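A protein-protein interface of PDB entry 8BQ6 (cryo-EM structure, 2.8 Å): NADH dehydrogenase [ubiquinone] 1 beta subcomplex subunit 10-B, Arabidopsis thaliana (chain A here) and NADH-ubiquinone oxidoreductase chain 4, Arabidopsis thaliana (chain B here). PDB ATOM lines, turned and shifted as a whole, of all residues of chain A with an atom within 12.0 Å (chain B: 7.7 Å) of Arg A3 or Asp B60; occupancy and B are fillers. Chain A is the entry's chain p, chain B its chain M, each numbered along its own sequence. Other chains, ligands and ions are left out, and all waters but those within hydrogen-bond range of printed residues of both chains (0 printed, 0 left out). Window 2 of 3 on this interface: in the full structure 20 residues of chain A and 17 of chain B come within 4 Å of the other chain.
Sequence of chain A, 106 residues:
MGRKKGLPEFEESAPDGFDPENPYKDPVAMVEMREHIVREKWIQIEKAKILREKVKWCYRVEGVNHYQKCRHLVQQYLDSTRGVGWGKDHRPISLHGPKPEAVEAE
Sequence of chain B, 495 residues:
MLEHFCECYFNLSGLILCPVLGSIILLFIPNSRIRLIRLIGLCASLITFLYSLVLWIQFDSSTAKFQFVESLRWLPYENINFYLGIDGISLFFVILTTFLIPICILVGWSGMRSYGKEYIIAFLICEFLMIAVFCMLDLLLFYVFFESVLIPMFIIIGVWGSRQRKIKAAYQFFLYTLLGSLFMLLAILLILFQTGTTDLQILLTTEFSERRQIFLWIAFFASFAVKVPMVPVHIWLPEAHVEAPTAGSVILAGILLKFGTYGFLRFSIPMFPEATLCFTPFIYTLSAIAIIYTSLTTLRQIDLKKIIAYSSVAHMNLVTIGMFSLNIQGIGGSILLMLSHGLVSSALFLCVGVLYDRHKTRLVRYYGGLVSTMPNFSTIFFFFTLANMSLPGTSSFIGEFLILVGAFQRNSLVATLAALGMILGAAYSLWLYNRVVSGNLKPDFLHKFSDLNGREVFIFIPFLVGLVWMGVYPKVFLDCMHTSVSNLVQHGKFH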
ATOM      1  N   GLY A   2      29.084  -4.706 -28.425  1.00  0.00           N
ATOM      2  CA  GLY A   2      28.862  -3.438 -29.095  1.00  0.00           C
ATOM      3  C   GLY A   2      27.404  -3.150 -29.386  1.00  0.00           C
ATOM      4  O   GLY A   2      26.600  -4.066 -29.549  1.00  0.00           O
ATOM      5  N   ARG A   3      27.070  -1.865 -29.455  1.00  0.00           N
ATOM      6  CA  ARG A   3      25.721  -1.399 -29.737  1.00  0.00           C
ATOM      7  C   ARG A   3      25.788  -0.253 -30.738  1.00  0.00           C
ATOM      8  O   ARG A   3      26.664   0.613 -30.646  1.00  0.00           O
ATOM      9  CB  ARG A   3      25.023  -0.955 -28.440  1.00  0.00           C
ATOM     10  CG  ARG A   3      24.053   0.200 -28.589  1.00  0.00           C
ATOM     11  CD  ARG A   3      23.474   0.617 -27.246  1.00  0.00           C
ATOM     12  NE  ARG A   3      22.488  -0.320 -26.726  1.00  0.00           N
ATOM     13  CZ  ARG A   3      21.199  -0.292 -27.035  1.00  0.00           C
ATOM     14  NH1 ARG A   3      20.716   0.580 -27.904  1.00  0.00           N
ATOM     15  NH2 ARG A   3      20.373  -1.155 -26.450  1.00  0.00           N
ATOM     16  N   LYS A   4      24.877  -0.263 -31.707  1.00  0.00           N
ATOM     17  CA  LYS A   4      24.815   0.811 -32.688  1.00  0.00           C
ATOM     18  C   LYS A   4      24.201   2.062 -32.078  1.00  0.00           C
ATOM     19  O   LYS A   4      23.319   1.995 -31.218  1.00  0.00           O
ATOM     20  CB  LYS A   4      24.002   0.383 -33.907  1.00  0.00           C
ATOM     21  CG  LYS A   4      23.962   1.430 -34.991  1.00  0.00           C
ATOM     22  CD  LYS A   4      23.386   0.889 -36.279  1.00  0.00           C
ATOM     23  CE  LYS A   4      21.896   0.656 -36.116  1.00  0.00           C
ATOM     24  NZ  LYS A   4      21.225   0.305 -37.393  1.00  0.00           N
ATOM     25  N   LYS A   5      24.671   3.213 -32.547  1.00  0.00           N
ATOM     26  CA  LYS A   5      24.158   4.486 -32.067  1.00  0.00           C
ATOM     27  C   LYS A   5      22.703   4.661 -32.481  1.00  0.00           C
ATOM     28  O   LYS A   5      22.247   4.085 -33.472  1.00  0.00           O
ATOM     29  CB  LYS A   5      25.013   5.632 -32.611  1.00  0.00           C
ATOM     30  CG  LYS A   5      24.697   7.001 -32.020  1.00  0.00           C
ATOM     31  CD  LYS A   5      25.816   8.005 -32.262  1.00  0.00           C
ATOM     32  CE  LYS A   5      26.573   7.716 -33.546  1.00  0.00           C
ATOM     33  NZ  LYS A   5      25.990   8.458 -34.699  1.00  0.00           N
ATOM     34  N   GLY A   6      21.967   5.442 -31.702  1.00  0.00           N
ATOM     35  CA  GLY A   6      20.595   5.780 -32.017  1.00  0.00           C
ATOM     36  C   GLY A   6      19.641   5.349 -30.923  1.00  0.00           C
ATOM     37  O   GLY A   6      20.007   4.695 -29.949  1.00  0.00           O
ATOM     38  N   LEU A   7      18.389   5.745 -31.109  1.00  0.00           N
ATOM     39  CA  LEU A   7      17.355   5.406 -30.153  1.00  0.00           C
ATOM     40  C   LEU A   7      17.052   3.909 -30.217  1.00  0.00           C
ATOM     41  O   LEU A   7      17.219   3.278 -31.264  1.00  0.00           O
ATOM     42  CB  LEU A   7      16.096   6.216 -30.437  1.00  0.00           C
ATOM     43  CG  LEU A   7      15.397   6.857 -29.238  1.00  0.00           C
ATOM     44  CD1 LEU A   7      16.271   7.923 -28.602  1.00  0.00           C
ATOM     45  CD2 LEU A   7      14.067   7.440 -29.668  1.00  0.00           C
ATOM     46  N   PRO A   8      16.626   3.313 -29.105  1.00  0.00           N
ATOM     47  CA  PRO A   8      16.260   1.891 -29.136  1.00  0.00           C
ATOM     48  C   PRO A   8      15.111   1.642 -30.099  1.00  0.00           C
ATOM     49  O   PRO A   8      14.240   2.492 -30.301  1.00  0.00           O
ATOM     50  CB  PRO A   8      15.859   1.580 -27.688  1.00  0.00           C
ATOM     51  CG  PRO A   8      15.894   2.849 -26.944  1.00  0.00           C
ATOM     52  CD  PRO A   8      16.546   3.903 -27.760  1.00  0.00           C
ATOM     53  N   GLU A   9      15.127   0.465 -30.715  1.00  0.00           N
ATOM     54  CA  GLU A   9      14.119   0.066 -31.688  1.00  0.00           C
ATOM     55  C   GLU A   9      13.334  -1.123 -31.157  1.00  0.00           C
ATOM     56  O   GLU A   9      13.922  -2.086 -30.654  1.00  0.00           O
ATOM     57  CB  GLU A   9      14.761  -0.288 -33.029  1.00  0.00           C
ATOM     58  CG  GLU A   9      14.659   0.810 -34.064  1.00  0.00           C
ATOM     59  CD  GLU A   9      13.237   1.295 -34.244  1.00  0.00           C
ATOM     60  OE1 GLU A   9      13.011   2.521 -34.159  1.00  0.00           O
ATOM     61  OE2 GLU A   9      12.345   0.449 -34.473  1.00  0.00           O
ATOM     62  N   PHE A  10      12.011  -1.058 -31.283  1.00  0.00           N
ATOM     63  CA  PHE A  10      11.125  -2.115 -30.820  1.00  0.00           C
ATOM     64  C   PHE A  10      10.053  -2.382 -31.868  1.00  0.00           C
ATOM     65  O   PHE A  10       9.749  -1.532 -32.709  1.00  0.00           O
ATOM     66  CB  PHE A  10      10.469  -1.761 -29.476  1.00  0.00           C
ATOM     67  CG  PHE A  10      11.446  -1.525 -28.352  1.00  0.00           C
ATOM     68  CD1 PHE A  10      12.064  -2.590 -27.714  1.00  0.00           C
ATOM     69  CD2 PHE A  10      11.718  -0.242 -27.911  1.00  0.00           C
ATOM     70  CE1 PHE A  10      12.950  -2.374 -26.674  1.00  0.00           C
ATOM     71  CE2 PHE A  10      12.599  -0.022 -26.872  1.00  0.00           C
ATOM     72  CZ  PHE A  10      13.216  -1.088 -26.253  1.00  0.00           C
ATOM     73  N   GLU A  35       6.244  -6.790 -22.019  1.00  0.00           N
ATOM     74  CA  GLU A  35       7.110  -5.682 -22.415  1.00  0.00           C
ATOM     75  C   GLU A  35       6.395  -4.729 -23.358  1.00  0.00           C
ATOM     76  O   GLU A  35       6.566  -3.507 -23.269  1.00  0.00           O
ATOM     77  CB  GLU A  35       8.376  -6.206 -23.086  1.00  0.00           C
ATOM     78  CG  GLU A  35       8.893  -7.491 -22.515  1.00  0.00           C
ATOM     79  CD  GLU A  35       9.993  -7.278 -21.520  1.00  0.00           C
ATOM     80  OE1 GLU A  35      10.161  -8.140 -20.634  1.00  0.00           O
ATOM     81  OE2 GLU A  35      10.696  -6.257 -21.640  1.00  0.00           O
ATOM     82  N   ARG A  39       5.628  -0.710 -22.769  1.00  0.00           N
ATOM     83  CA  ARG A  39       6.003   0.324 -23.725  1.00  0.00           C
ATOM     84  C   ARG A  39       4.788   1.105 -24.195  1.00  0.00           C
ATOM     85  O   ARG A  39       4.852   2.329 -24.360  1.00  0.00           O
ATOM     86  CB  ARG A  39       6.724  -0.306 -24.910  1.00  0.00           C
ATOM     87  CG  ARG A  39       8.152  -0.686 -24.618  1.00  0.00           C
ATOM     88  CD  ARG A  39       8.797  -1.240 -25.857  1.00  0.00           C
ATOM     89  NE  ARG A  39       9.142  -2.647 -25.711  1.00  0.00           N
ATOM     90  CZ  ARG A  39       8.670  -3.614 -26.484  1.00  0.00           C
ATOM     91  NH1 ARG A  39       7.790  -3.367 -27.440  1.00  0.00           N
ATOM     92  NH2 ARG A  39       9.095  -4.859 -26.296  1.00  0.00           N
ATOM     93  N   LEU B  55      30.407  -1.099 -14.590  1.00  0.00           N
ATOM     94  CA  LEU B  55      29.127  -1.779 -14.815  1.00  0.00           C
ATOM     95  C   LEU B  55      27.966  -0.798 -14.922  1.00  0.00           C
ATOM     96  O   LEU B  55      27.084  -0.962 -15.775  1.00  0.00           O
ATOM     97  CB  LEU B  55      28.849  -2.778 -13.702  1.00  0.00           C
ATOM     98  CG  LEU B  55      29.235  -4.230 -13.919  1.00  0.00           C
ATOM     99  CD1 LEU B  55      30.714  -4.397 -13.884  1.00  0.00           C
ATOM    100  CD2 LEU B  55      28.603  -4.998 -12.787  1.00  0.00           C
ATOM    101  N   TRP B  56      27.924   0.203 -14.047  1.00  0.00           N
ATOM    102  CA  TRP B  56      26.931   1.256 -14.238  1.00  0.00           C
ATOM    103  C   TRP B  56      27.050   1.870 -15.627  1.00  0.00           C
ATOM    104  O   TRP B  56      26.044   2.061 -16.317  1.00  0.00           O
ATOM    105  CB  TRP B  56      27.073   2.341 -13.175  1.00  0.00           C
ATOM    106  CG  TRP B  56      25.944   3.324 -13.179  1.00  0.00           C
ATOM    107  CD1 TRP B  56      24.885   3.361 -14.040  1.00  0.00           C
ATOM    108  CD2 TRP B  56      25.791   4.447 -12.313  1.00  0.00           C
ATOM    109  NE1 TRP B  56      24.073   4.424 -13.747  1.00  0.00           N
ATOM    110  CE2 TRP B  56      24.607   5.107 -12.689  1.00  0.00           C
ATOM    111  CE3 TRP B  56      26.534   4.949 -11.244  1.00  0.00           C
ATOM    112  CZ2 TRP B  56      24.151   6.242 -12.035  1.00  0.00           C
ATOM    113  CZ3 TRP B  56      26.081   6.072 -10.597  1.00  0.00           C
ATOM    114  CH2 TRP B  56      24.899   6.709 -10.992  1.00  0.00           C
ATOM    115  N   ILE B  57      28.277   2.162 -16.064  1.00  0.00           N
ATOM    116  CA  ILE B  57      28.456   2.937 -17.293  1.00  0.00           C
ATOM    117  C   ILE B  57      27.873   2.207 -18.505  1.00  0.00           C
ATOM    118  O   ILE B  57      27.296   2.835 -19.401  1.00  0.00           O
ATOM    119  CB  ILE B  57      29.943   3.292 -17.483  1.00  0.00           C
ATOM    120  CG1 ILE B  57      30.315   4.471 -16.585  1.00  0.00           C
ATOM    121  CG2 ILE B  57      30.243   3.659 -18.921  1.00  0.00           C
ATOM    122  CD1 ILE B  57      29.194   5.463 -16.375  1.00  0.00           C
ATOM    123  N   GLN B  58      27.990   0.881 -18.552  1.00  0.00           N
ATOM    124  CA  GLN B  58      27.512   0.116 -19.698  1.00  0.00           C
ATOM    125  C   GLN B  58      26.079  -0.382 -19.530  1.00  0.00           C
ATOM    126  O   GLN B  58      25.622  -1.211 -20.326  1.00  0.00           O
ATOM    127  CB  GLN B  58      28.443  -1.062 -19.966  1.00  0.00           C
ATOM    128  CG  GLN B  58      28.960  -1.690 -18.708  1.00  0.00           C
ATOM    129  CD  GLN B  58      29.738  -2.946 -18.975  1.00  0.00           C
ATOM    130  OE1 GLN B  58      30.789  -2.911 -19.609  1.00  0.00           O
ATOM    131  NE2 GLN B  58      29.230  -4.069 -18.489  1.00  0.00           N
ATOM    132  N   PHE B  59      25.367   0.098 -18.518  1.00  0.00           N
ATOM    133  CA  PHE B  59      23.998  -0.330 -18.285  1.00  0.00           C
ATOM    134  C   PHE B  59      23.074   0.169 -19.387  1.00  0.00           C
ATOM    135  O   PHE B  59      23.211   1.295 -19.873  1.00  0.00           O
ATOM    136  CB  PHE B  59      23.510   0.173 -16.932  1.00  0.00           C
ATOM    137  CG  PHE B  59      22.182  -0.373 -16.533  1.00  0.00           C
ATOM    138  CD1 PHE B  59      22.065  -1.670 -16.075  1.00  0.00           C
ATOM    139  CD2 PHE B  59      21.047   0.414 -16.607  1.00  0.00           C
ATOM    140  CE1 PHE B  59      20.845  -2.172 -15.699  1.00  0.00           C
ATOM    141  CE2 PHE B  59      19.823  -0.086 -16.236  1.00  0.00           C
ATOM    142  CZ  PHE B  59      19.721  -1.379 -15.779  1.00  0.00           C
ATOM    143  N   ASP B  60      22.126  -0.676 -19.772  1.00  0.00           N
ATOM    144  CA  ASP B  60      21.170  -0.376 -20.831  1.00  0.00           C
ATOM    145  C   ASP B  60      19.803  -0.208 -20.182  1.00  0.00           C
ATOM    146  O   ASP B  60      19.263  -1.156 -19.602  1.00  0.00           O
ATOM    147  CB  ASP B  60      21.172  -1.484 -21.881  1.00  0.00           C
ATOM    148  CG  ASP B  60      20.018  -1.371 -22.856  1.00  0.00           C
ATOM    149  OD1 ASP B  60      19.592  -0.240 -23.156  1.00  0.00           O
ATOM    150  OD2 ASP B  60      19.542  -2.420 -23.333  1.00  0.00           O
ATOM    151  N   SER B  61      19.247   0.998 -20.278  1.00  0.00           N
ATOM    152  CA  SER B  61      18.066   1.382 -19.520  1.00  0.00           C
ATOM    153  C   SER B  61      16.780   1.304 -20.337  1.00  0.00           C
ATOM    154  O   SER B  61      15.726   1.746 -19.866  1.00  0.00           O
ATOM    155  CB  SER B  61      18.265   2.783 -18.940  1.00  0.00           C
ATOM    156  OG  SER B  61      18.254   3.765 -19.956  1.00  0.00           O
ATOM    157  N   SER B  62      16.842   0.737 -21.542  1.00  0.00           N
ATOM    158  CA  SER B  62      15.661   0.514 -22.360  1.00  0.00           C
ATOM    159  C   SER B  62      15.113  -0.900 -22.273  1.00  0.00           C
ATOM    160  O   SER B  62      13.994  -1.137 -22.734  1.00  0.00           O
ATOM    161  CB  SER B  62      15.964   0.828 -23.831  1.00  0.00           C
ATOM    162  OG  SER B  62      16.848  -0.132 -24.379  1.00  0.00           O
ATOM    163  N   THR B  63      15.861  -1.837 -21.708  1.00  0.00           N
ATOM    164  CA  THR B  63      15.435  -3.224 -21.711  1.00  0.00           C
ATOM    165  C   THR B  63      14.853  -3.604 -20.360  1.00  0.00           C
ATOM    166  O   THR B  63      15.291  -3.125 -19.311  1.00  0.00           O
ATOM    167  CB  THR B  63      16.599  -4.161 -22.042  1.00  0.00           C
ATOM    168  OG1 THR B  63      16.185  -5.517 -21.850  1.00  0.00           O
ATOM    169  CG2 THR B  63      17.771  -3.894 -21.125  1.00  0.00           C
ATOM    170  N   ALA B  64      13.842  -4.461 -20.396  1.00  0.00           N
ATOM    171  CA  ALA B  64      13.365  -5.088 -19.177  1.00  0.00           C
ATOM    172  C   ALA B  64      13.983  -6.456 -18.949  1.00  0.00           C
ATOM    173  O   ALA B  64      13.711  -7.077 -17.917  1.00  0.00           O
ATOM    174  CB  ALA B  64      11.848  -5.215 -19.200  1.00  0.00           C
ATOM    175  N   LYS B  65      14.798  -6.933 -19.882  1.00  0.00           N
ATOM    176  CA  LYS B  65      15.488  -8.198 -19.713  1.00  0.00           C
ATOM    177  C   LYS B  65      16.610  -8.040 -18.691  1.00  0.00           C
ATOM    178  O   LYS B  65      17.011  -6.931 -18.329  1.00  0.00           O
ATOM    179  CB  LYS B  65      16.032  -8.692 -21.051  1.00  0.00           C
ATOM    180  CG  LYS B  65      15.044  -9.492 -21.892  1.00  0.00           C
ATOM    181  CD  LYS B  65      14.050  -8.592 -22.612  1.00  0.00           C
ATOM    182  CE  LYS B  65      12.813  -9.358 -23.058  1.00  0.00           C
ATOM    183  NZ  LYS B  65      12.267  -8.811 -24.331  1.00  0.00           N
ATOM    184  N   GLN B  67      20.390  -8.019 -17.691  1.00  0.00           N
ATOM    185  CA  GLN B  67      21.557  -7.593 -18.445  1.00  0.00           C
ATOM    186  C   GLN B  67      22.825  -8.242 -17.909  1.00  0.00           C
ATOM    187  O   GLN B  67      22.876  -8.731 -16.778  1.00  0.00           O
ATOM    188  CB  GLN B  67      21.698  -6.072 -18.415  1.00  0.00           C
ATOM    189  CG  GLN B  67      20.458  -5.366 -18.877  1.00  0.00           C
ATOM    190  CD  GLN B  67      20.578  -3.875 -18.789  1.00  0.00           C
ATOM    191  OE1 GLN B  67      21.598  -3.297 -19.157  1.00  0.00           O
ATOM    192  NE2 GLN B  67      19.525  -3.234 -18.309  1.00  0.00           N
ATOM    193  N   PHE B  68      23.855  -8.239 -18.756  1.00  0.00           N
ATOM    194  CA  PHE B  68      25.144  -8.865 -18.468  1.00  0.00           C
ATOM    195  C   PHE B  68      24.972 -10.306 -18.007  1.00  0.00           C
ATOM    196  O   PHE B  68      25.754 -10.801 -17.192  1.00  0.00           O
ATOM    197  CB  PHE B  68      25.937  -8.059 -17.432  1.00  0.00           C
ATOM    198  CG  PHE B  68      25.893  -6.573 -17.657  1.00  0.00           C
ATOM    199  CD1 PHE B  68      26.094  -6.042 -18.918  1.00  0.00           C
ATOM    200  CD2 PHE B  68      25.634  -5.708 -16.610  1.00  0.00           C
ATOM    201  CE1 PHE B  68      26.044  -4.683 -19.125  1.00  0.00           C
ATOM    202  CE2 PHE B  68      25.582  -4.347 -16.817  1.00  0.00           C
ATOM    203  CZ  PHE B  68      25.787  -3.837 -18.074  1.00  0.00           C
ATOM    204  N   ILE B  86      21.799  -8.637 -13.715  1.00  0.00           N
ATOM    205  CA  ILE B  86      21.234  -7.536 -12.954  1.00  0.00           C
ATOM    206  C   ILE B  86      20.246  -6.765 -13.814  1.00  0.00           C
ATOM    207  O   ILE B  86      20.262  -6.855 -15.046  1.00  0.00           O
ATOM    208  CB  ILE B  86      22.341  -6.613 -12.418  1.00  0.00           C
ATOM    209  CG1 ILE B  86      23.252  -6.157 -13.552  1.00  0.00           C
ATOM    210  CG2 ILE B  86      23.173  -7.340 -11.370  1.00  0.00           C
ATOM    211  CD1 ILE B  86      24.514  -5.505 -13.061  1.00  0.00           C
ATOM    212  N   ASP B  87      19.375  -6.006 -13.166  1.00  0.00           N
ATOM    213  CA  ASP B  87      18.493  -5.098 -13.876  1.00  0.00           C
ATOM    214  C   ASP B  87      18.509  -3.777 -13.117  1.00  0.00           C
ATOM    215  O   ASP B  87      19.368  -3.554 -12.257  1.00  0.00           O
ATOM    216  CB  ASP B  87      17.096  -5.725 -14.041  1.00  0.00           C
ATOM    217  CG  ASP B  87      16.487  -6.163 -12.726  1.00  0.00           C
ATOM    218  OD1 ASP B  87      16.127  -7.347 -12.599  1.00  0.00           O
ATOM    219  OD2 ASP B  87      16.344  -5.325 -11.821  1.00  0.00           O
ATOM    220  N   GLY B  88      17.577  -2.891 -13.444  1.00  0.00           N
ATOM    221  CA  GLY B  88      17.506  -1.617 -12.766  1.00  0.00           C
ATOM    222  C   GLY B  88      17.183  -1.691 -11.295  1.00  0.00           C
ATOM    223  O   GLY B  88      17.349  -0.701 -10.579  1.00  0.00           O
ATOM    224  N   ASP B 479      16.090   7.183 -14.063  1.00  0.00           N
ATOM    225  CA  ASP B 479      16.110   6.853 -15.485  1.00  0.00           C
ATOM    226  C   ASP B 479      16.561   5.418 -15.721  1.00  0.00           C
ATOM    227  O   ASP B 479      16.009   4.719 -16.580  1.00  0.00           O
ATOM    228  CB  ASP B 479      17.029   7.811 -16.233  1.00  0.00           C
ATOM    229  CG  ASP B 479      16.337   9.090 -16.630  1.00  0.00           C
ATOM    230  OD1 ASP B 479      15.105   9.192 -16.448  1.00  0.00           O
ATOM    231  OD2 ASP B 479      17.032   9.997 -17.130  1.00  0.00           O
ATOM    232  N   CYS B 480      17.574   4.967 -14.985  1.00  0.00           N
ATOM    233  CA  CYS B 480      18.100   3.624 -15.168  1.00  0.00           C
ATOM    234  C   CYS B 480      17.220   2.555 -14.542  1.00  0.00           C
ATOM    235  O   CYS B 480      17.507   1.366 -14.705  1.00  0.00           O
ATOM    236  CB  CYS B 480      19.512   3.526 -14.586  1.00  0.00           C
ATOM    237  SG  CYS B 480      20.761   4.485 -15.475  1.00  0.00           S
ATOM    238  N   THR B 483      12.396   1.220 -16.434  1.00  0.00           N
ATOM    239  CA  THR B 483      11.992   0.134 -17.322  1.00  0.00           C
ATOM    240  C   THR B 483      11.823  -1.169 -16.550  1.00  0.00           C
ATOM    241  O   THR B 483      10.886  -1.935 -16.797  1.00  0.00           O
ATOM    242  CB  THR B 483      13.007  -0.039 -18.448  1.00  0.00           C
ATOM    243  OG1 THR B 483      13.251   1.227 -19.070  1.00  0.00           O
ATOM    244  CG2 THR B 483      12.468  -1.004 -19.485  1.00  0.00           C
ATOM    245  N   SER B 484      12.741  -1.441 -15.619  1.00  0.00           N
ATOM    246  CA  SER B 484      12.612  -2.609 -14.755  1.00  0.00           C
ATOM    247  C   SER B 484      11.472  -2.434 -13.762  1.00  0.00           C
ATOM    248  O   SER B 484      10.757  -3.390 -13.442  1.00  0.00           O
ATOM    249  CB  SER B 484      13.925  -2.856 -14.016  1.00  0.00           C
ATOM    250  OG  SER B 484      14.960  -3.199 -14.915  1.00  0.00           O
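OD2 of Asp B60 lies within salt-bridge range of NH2 of Arg A3 (3.5 Å).
The backbone carbonyl oxygen (O) of Asp B60 is in hydrogen-bond range of the side-chain amide nitrogen (NE2) of Gln B67 (2.5 Å).
The side-chain hydroxyl (OG1) of Thr B63 is in hydrogen-bond range of the backbone NH (N) of Lys B65, at 2.8 Å.
OD1 of Asp B60 sits at hydrogen-bond distance from OG of Ser B62, at 3.0 Å.
Pro A8 touches Ser B62.
Phe A10 touches Ser B62 (CZ to O, 3.6 Å).
Glu A35 touches Ala B64 (OE2 to CB, 2.9 Å).
Glu A35 touches Lys B65.
Of chain B, only Asp B60 comes within 4 Å of Arg A3.
Of chain A, only Arg A3 comes within 4 Å of Asp B60.
No residue of chain B comes within 4 Å of Gly A2.
No residue of chain A comes within 4 Å of Phe B59.
No residue of chain A comes within 4 Å of Ser B61.
No residue of chain A comes within 4 Å of Thr B63.
No residue of chain A comes within 4 Å of Cys B480.
Of the printed residues of chain A, Lys B65 touches Glu A35.
Printed residues of chain B within 4 Å of Glu A35: Ala B64 and Lys B65.
The nearest residue of chain B that does not touch Arg A3 is Ser B62 (4.2 Å).
The nearest residue of chain A that does not touch Asp B60 is Pro A8 (6.1 Å).
Of the 20 printed residues of chain B, 4 touch a printed residue of chain A.
Printed residues of chain A that touch a printed residue of chain B: Arg A3, Pro A8, Phe A10 and Glu A35.
Hydrophobic or aromatic side chains of chain A within 4 Å of the printed part of chain B: Pro A8 and Phe A10.
Among the printed residues, 5 pairs touch across the chains.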
